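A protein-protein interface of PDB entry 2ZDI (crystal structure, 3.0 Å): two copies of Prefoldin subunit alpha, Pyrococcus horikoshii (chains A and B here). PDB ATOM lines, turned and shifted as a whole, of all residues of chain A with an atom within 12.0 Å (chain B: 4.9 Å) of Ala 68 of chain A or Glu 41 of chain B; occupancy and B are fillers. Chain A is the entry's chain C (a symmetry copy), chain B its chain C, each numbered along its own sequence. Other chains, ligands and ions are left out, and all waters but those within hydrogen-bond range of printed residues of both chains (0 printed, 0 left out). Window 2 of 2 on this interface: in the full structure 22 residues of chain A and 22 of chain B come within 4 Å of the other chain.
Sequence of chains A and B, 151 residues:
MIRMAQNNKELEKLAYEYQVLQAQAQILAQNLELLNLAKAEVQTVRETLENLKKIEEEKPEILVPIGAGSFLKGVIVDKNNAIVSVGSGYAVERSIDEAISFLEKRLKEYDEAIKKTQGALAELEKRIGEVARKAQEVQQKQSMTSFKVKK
The backbone carbonyl oxygen of Gly 69 of chain A lies within hydrogen-bond range of the backbone NH of Ser 85 of chain B.
O of Ala 68 of chain A is in hydrogen-bond range of OG of Ser 70 of chain A (3.0 Å).
Val 45 of chain B touches Ile 66 of chain A.
C of Gly 67 of chain A touches OE2 of Glu 41 of chain B (3.9 Å).
Val 45 of chain B touches Gly 67 of chain A.
Glu 41 of chain B touches Ala 68 of chain A (OE2 to N, 3.8 Å).
Ala 68 of chain A touches Val 45 of chain B.
C of Val 84 of chain B touches O of Gly 69 of chain A, 3.5 Å away.
OG of Ser 70 of chain A touches CG1 of Val 45 of chain B, at 3.4 Å.
Of the printed residues of chain B, Ile 66 of chain A touches Val 45 (3.4 Å).
Printed residues of chain B within 4 Å of Gly 67 of chain A: Glu 41 and Val 45.
Of chain B, only Glu 41 (3.8 Å) and Val 45 (3.3 Å) come within 4 Å of Ala 68 of chain A.
Of the printed residues of chain B, Gly 69 of chain A touches Val 84 (3.5 Å) and Ser 85 (2.9 Å).
Printed residues of chain B within 4 Å of Ser 70 of chain A: Val 45.
Of chain A, only Gly 67 (3.9 Å) and Ala 68 (3.8 Å) come within 4 Å of Glu 41 of chain B.
No residue of chain A comes within 4 Å of Gln 43 of chain B.
Of chain A, only Gly 69 (3.5 Å) comes within 4 Å of Val 84 of chain B.
Of the printed residues of chain A, Ser 85 of chain B touches Gly 69 (2.9 Å).
The nearest printed residue of chain B that does not touch Ile 66 of chain A is Thr 44 of chain B (5.3 Å).
Hydrophobic or aromatic side chains of chain B that line the printed part of chain A: Val 45.
Hydrophobic or aromatic side chains of chain A within 4 Å of the printed part of chain B: Ile 66.
Among the printed residues, no Asp or Glu carboxylate lies within 4 Å of a Lys or Arg side-chain nitrogen of the other chain.
No position is printed for both chains.
Of the 8 pairs that touch across the chains among the printed residues, none has its exchanged pair printed and touching as well.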
ATOM      1  N   LEU A  63      14.741  29.677  -3.615  1.00  0.00           N
ATOM      2  CA  LEU A  63      13.543  29.085  -4.198  1.00  0.00           C
ATOM      3  C   LEU A  63      12.855  30.143  -5.042  1.00  0.00           C
ATOM      4  O   LEU A  63      12.468  31.198  -4.535  1.00  0.00           O
ATOM      5  CB  LEU A  63      12.585  28.584  -3.117  1.00  0.00           C
ATOM      6  CG  LEU A  63      12.704  27.109  -2.740  1.00  0.00           C
ATOM      7  CD1 LEU A  63      14.156  26.684  -2.723  1.00  0.00           C
ATOM      8  CD2 LEU A  63      12.044  26.849  -1.399  1.00  0.00           C
ATOM      9  N   VAL A  64      12.722  29.871  -6.337  1.00  0.00           N
ATOM     10  CA  VAL A  64      12.045  30.799  -7.234  1.00  0.00           C
ATOM     11  C   VAL A  64      10.566  30.443  -7.382  1.00  0.00           C
ATOM     12  O   VAL A  64      10.224  29.363  -7.878  1.00  0.00           O
ATOM     13  CB  VAL A  64      12.751  30.903  -8.611  1.00  0.00           C
ATOM     14  CG1 VAL A  64      13.590  29.663  -8.886  1.00  0.00           C
ATOM     15  CG2 VAL A  64      11.741  31.162  -9.726  1.00  0.00           C
ATOM     16  N   PRO A  65       9.684  31.341  -6.931  1.00  0.00           N
ATOM     17  CA  PRO A  65       8.232  31.162  -6.940  1.00  0.00           C
ATOM     18  C   PRO A  65       7.684  31.206  -8.361  1.00  0.00           C
ATOM     19  O   PRO A  65       7.924  32.177  -9.078  1.00  0.00           O
ATOM     20  CB  PRO A  65       7.715  32.362  -6.140  1.00  0.00           C
ATOM     21  CG  PRO A  65       8.913  32.906  -5.420  1.00  0.00           C
ATOM     22  CD  PRO A  65      10.065  32.631  -6.316  1.00  0.00           C
ATOM     23  N   ILE A  66       6.962  30.172  -8.764  1.00  0.00           N
ATOM     24  CA  ILE A  66       6.471  30.103 -10.129  1.00  0.00           C
ATOM     25  C   ILE A  66       4.956  30.071 -10.176  1.00  0.00           C
ATOM     26  O   ILE A  66       4.370  29.921 -11.243  1.00  0.00           O
ATOM     27  CB  ILE A  66       7.016  28.874 -10.861  1.00  0.00           C
ATOM     28  CG1 ILE A  66       6.609  27.599 -10.118  1.00  0.00           C
ATOM     29  CG2 ILE A  66       8.526  28.976 -11.002  1.00  0.00           C
ATOM     30  CD1 ILE A  66       6.679  26.339 -10.958  1.00  0.00           C
ATOM     31  N   GLY A  67       4.319  30.204  -9.021  1.00  0.00           N
ATOM     32  CA  GLY A  67       2.873  30.228  -8.991  1.00  0.00           C
ATOM     33  C   GLY A  67       2.262  29.710  -7.711  1.00  0.00           C
ATOM     34  O   GLY A  67       2.723  30.036  -6.618  1.00  0.00           O
ATOM     35  N   ALA A  68       1.223  28.895  -7.856  1.00  0.00           N
ATOM     36  CA  ALA A  68       0.412  28.459  -6.725  1.00  0.00           C
ATOM     37  C   ALA A  68       1.139  27.485  -5.798  1.00  0.00           C
ATOM     38  O   ALA A  68       1.060  26.271  -5.976  1.00  0.00           O
ATOM     39  CB  ALA A  68      -0.889  27.848  -7.223  1.00  0.00           C
ATOM     40  N   GLY A  69       1.836  28.025  -4.801  1.00  0.00           N
ATOM     41  CA  GLY A  69       2.576  27.214  -3.850  1.00  0.00           C
ATOM     42  C   GLY A  69       3.711  26.442  -4.493  1.00  0.00           C
ATOM     43  O   GLY A  69       4.273  25.525  -3.894  1.00  0.00           O
ATOM     44  N   SER A  70       4.052  26.824  -5.718  1.00  0.00           N
ATOM     45  CA  SER A  70       5.045  26.104  -6.492  1.00  0.00           C
ATOM     46  C   SER A  70       6.354  26.872  -6.546  1.00  0.00           C
ATOM     47  O   SER A  70       6.363  28.095  -6.691  1.00  0.00           O
ATOM     48  CB  SER A  70       4.528  25.862  -7.904  1.00  0.00           C
ATOM     49  OG  SER A  70       3.180  25.437  -7.869  1.00  0.00           O
ATOM     50  N   PHE A  71       7.455  26.138  -6.429  1.00  0.00           N
ATOM     51  CA  PHE A  71       8.782  26.727  -6.396  1.00  0.00           C
ATOM     52  C   PHE A  71       9.749  25.868  -7.172  1.00  0.00           C
ATOM     53  O   PHE A  71       9.547  24.667  -7.323  1.00  0.00           O
ATOM     54  CB  PHE A  71       9.280  26.850  -4.956  1.00  0.00           C
ATOM     55  CG  PHE A  71       8.389  27.673  -4.090  1.00  0.00           C
ATOM     56  CD1 PHE A  71       8.653  29.015  -3.889  1.00  0.00           C
ATOM     57  CD2 PHE A  71       7.272  27.112  -3.495  1.00  0.00           C
ATOM     58  CE1 PHE A  71       7.828  29.783  -3.098  1.00  0.00           C
ATOM     59  CE2 PHE A  71       6.439  27.873  -2.705  1.00  0.00           C
ATOM     60  CZ  PHE A  71       6.719  29.213  -2.503  1.00  0.00           C
ATOM     61  N   LEU A  72      10.806  26.496  -7.663  1.00  0.00           N
ATOM     62  CA  LEU A  72      11.879  25.763  -8.303  1.00  0.00           C
ATOM     63  C   LEU A  72      13.168  26.044  -7.548  1.00  0.00           C
ATOM     64  O   LEU A  72      13.279  27.045  -6.840  1.00  0.00           O
ATOM     65  CB  LEU A  72      12.004  26.147  -9.779  1.00  0.00           C
ATOM     66  CG  LEU A  72      10.825  25.811 -10.699  1.00  0.00           C
ATOM     67  CD1 LEU A  72      11.177  26.156 -12.125  1.00  0.00           C
ATOM     68  CD2 LEU A  72      10.431  24.345 -10.601  1.00  0.00           C
ATOM     69  N   LEU B  37     -10.210  32.757 -11.782  1.00  0.00           N
ATOM     70  CA  LEU B  37      -8.912  33.426 -11.746  1.00  0.00           C
ATOM     71  C   LEU B  37      -7.846  32.544 -11.103  1.00  0.00           C
ATOM     72  O   LEU B  37      -6.746  32.398 -11.634  1.00  0.00           O
ATOM     73  CB  LEU B  37      -9.000  34.764 -11.010  1.00  0.00           C
ATOM     74  CG  LEU B  37      -9.538  35.947 -11.816  1.00  0.00           C
ATOM     75  CD1 LEU B  37      -9.424  37.228 -11.006  1.00  0.00           C
ATOM     76  CD2 LEU B  37      -8.808  36.083 -13.148  1.00  0.00           C
ATOM     77  N   ALA B  38      -8.173  31.963  -9.956  1.00  0.00           N
ATOM     78  CA  ALA B  38      -7.270  31.026  -9.303  1.00  0.00           C
ATOM     79  C   ALA B  38      -6.984  29.848 -10.228  1.00  0.00           C
ATOM     80  O   ALA B  38      -5.852  29.378 -10.312  1.00  0.00           O
ATOM     81  CB  ALA B  38      -7.860  30.547  -7.990  1.00  0.00           C
ATOM     82  N   LYS B  39      -8.012  29.380 -10.927  1.00  0.00           N
ATOM     83  CA  LYS B  39      -7.843  28.292 -11.882  1.00  0.00           C
ATOM     84  C   LYS B  39      -6.943  28.707 -13.044  1.00  0.00           C
ATOM     85  O   LYS B  39      -6.175  27.897 -13.564  1.00  0.00           O
ATOM     86  CB  LYS B  39      -9.191  27.802 -12.418  1.00  0.00           C
ATOM     87  CG  LYS B  39      -9.043  26.803 -13.559  1.00  0.00           C
ATOM     88  CD  LYS B  39     -10.370  26.344 -14.130  1.00  0.00           C
ATOM     89  CE  LYS B  39     -10.147  25.324 -15.242  1.00  0.00           C
ATOM     90  NZ  LYS B  39     -11.415  24.896 -15.888  1.00  0.00           N
ATOM     91  N   ALA B  40      -7.045  29.967 -13.453  1.00  0.00           N
ATOM     92  CA  ALA B  40      -6.224  30.476 -14.547  1.00  0.00           C
ATOM     93  C   ALA B  40      -4.765  30.606 -14.117  1.00  0.00           C
ATOM     94  O   ALA B  40      -3.855  30.482 -14.941  1.00  0.00           O
ATOM     95  CB  ALA B  40      -6.760  31.810 -15.042  1.00  0.00           C
ATOM     96  N   GLU B  41      -4.553  30.858 -12.825  1.00  0.00           N
ATOM     97  CA  GLU B  41      -3.207  30.911 -12.259  1.00  0.00           C
ATOM     98  C   GLU B  41      -2.596  29.518 -12.200  1.00  0.00           C
ATOM     99  O   GLU B  41      -1.443  29.317 -12.574  1.00  0.00           O
ATOM    100  CB  GLU B  41      -3.219  31.522 -10.857  1.00  0.00           C
ATOM    101  CG  GLU B  41      -1.866  31.435 -10.154  1.00  0.00           C
ATOM    102  CD  GLU B  41      -1.881  31.998  -8.739  1.00  0.00           C
ATOM    103  OE1 GLU B  41      -2.979  32.301  -8.225  1.00  0.00           O
ATOM    104  OE2 GLU B  41      -0.790  32.136  -8.141  1.00  0.00           O
ATOM    105  N   VAL B  42      -3.378  28.558 -11.719  1.00  0.00           N
ATOM    106  CA  VAL B  42      -2.944  27.167 -11.673  1.00  0.00           C
ATOM    107  C   VAL B  42      -2.580  26.669 -13.073  1.00  0.00           C
ATOM    108  O   VAL B  42      -1.577  25.982 -13.255  1.00  0.00           O
ATOM    109  CB  VAL B  42      -4.028  26.261 -11.044  1.00  0.00           C
ATOM    110  CG1 VAL B  42      -3.598  24.808 -11.079  1.00  0.00           C
ATOM    111  CG2 VAL B  42      -4.323  26.695  -9.614  1.00  0.00           C
ATOM    112  N   GLN B  43      -3.391  27.032 -14.062  1.00  0.00           N
ATOM    113  CA  GLN B  43      -3.137  26.633 -15.441  1.00  0.00           C
ATOM    114  C   GLN B  43      -1.827  27.209 -15.956  1.00  0.00           C
ATOM    115  O   GLN B  43      -1.174  26.609 -16.808  1.00  0.00           O
ATOM    116  CB  GLN B  43      -4.294  27.045 -16.356  1.00  0.00           C
ATOM    117  CG  GLN B  43      -5.335  25.951 -16.561  1.00  0.00           C
ATOM    118  CD  GLN B  43      -6.652  26.474 -17.113  1.00  0.00           C
ATOM    119  OE1 GLN B  43      -6.875  27.684 -17.183  1.00  0.00           O
ATOM    120  NE2 GLN B  43      -7.537  25.558 -17.500  1.00  0.00           N
ATOM    121  N   THR B  44      -1.443  28.369 -15.435  1.00  0.00           N
ATOM    122  CA  THR B  44      -0.215  29.022 -15.880  1.00  0.00           C
ATOM    123  C   THR B  44       1.015  28.459 -15.163  1.00  0.00           C
ATOM    124  O   THR B  44       2.101  28.390 -15.741  1.00  0.00           O
ATOM    125  CB  THR B  44      -0.285  30.561 -15.731  1.00  0.00           C
ATOM    126  OG1 THR B  44       0.537  31.175 -16.729  1.00  0.00           O
ATOM    127  CG2 THR B  44       0.187  31.003 -14.354  1.00  0.00           C
ATOM    128  N   VAL B  45       0.843  28.051 -13.909  1.00  0.00           N
ATOM    129  CA  VAL B  45       1.915  27.386 -13.179  1.00  0.00           C
ATOM    130  C   VAL B  45       2.132  25.999 -13.768  1.00  0.00           C
ATOM    131  O   VAL B  45       3.233  25.454 -13.710  1.00  0.00           O
ATOM    132  CB  VAL B  45       1.602  27.255 -11.681  1.00  0.00           C
ATOM    133  CG1 VAL B  45       2.857  26.873 -10.915  1.00  0.00           C
ATOM    134  CG2 VAL B  45       1.026  28.551 -11.151  1.00  0.00           C
ATOM    135  N   VAL B  84       5.743  21.686  -4.786  1.00  0.00           N
ATOM    136  CA  VAL B  84       4.347  22.071  -4.900  1.00  0.00           C
ATOM    137  C   VAL B  84       3.691  22.058  -3.529  1.00  0.00           C
ATOM    138  O   VAL B  84       3.905  21.143  -2.735  1.00  0.00           O
ATOM    139  CB  VAL B  84       3.586  21.122  -5.834  1.00  0.00           C
ATOM    140  CG1 VAL B  84       2.264  21.741  -6.252  1.00  0.00           C
ATOM    141  CG2 VAL B  84       4.428  20.805  -7.050  1.00  0.00           C
ATOM    142  N   SER B  85       2.890  23.079  -3.253  1.00  0.00           N
ATOM    143  CA  SER B  85       2.249  23.206  -1.955  1.00  0.00           C
ATOM    144  C   SER B  85       1.156  22.157  -1.735  1.00  0.00           C
ATOM    145  O   SER B  85       0.202  22.069  -2.506  1.00  0.00           O
ATOM    146  CB  SER B  85       1.676  24.610  -1.784  1.00  0.00           C
ATOM    147  OG  SER B  85       1.168  24.789  -0.476  1.00  0.00           O
ATOM    148  N   LEU B 103      -1.040  19.346  -9.979  1.00  0.00           N
ATOM    149  CA  LEU B 103      -1.605  20.637 -10.351  1.00  0.00           C
ATOM    150  C   LEU B 103      -2.885  20.473 -11.152  1.00  0.00           C
ATOM    151  O   LEU B 103      -3.831  21.240 -10.981  1.00  0.00           O
ATOM    152  CB  LEU B 103      -0.602  21.460 -11.155  1.00  0.00           C
ATOM    153  CG  LEU B 103       0.487  22.157 -10.343  1.00  0.00           C
ATOM    154  CD1 LEU B 103       1.354  22.998 -11.260  1.00  0.00           C
ATOM    155  CD2 LEU B 103      -0.135  23.010  -9.253  1.00  0.00           C
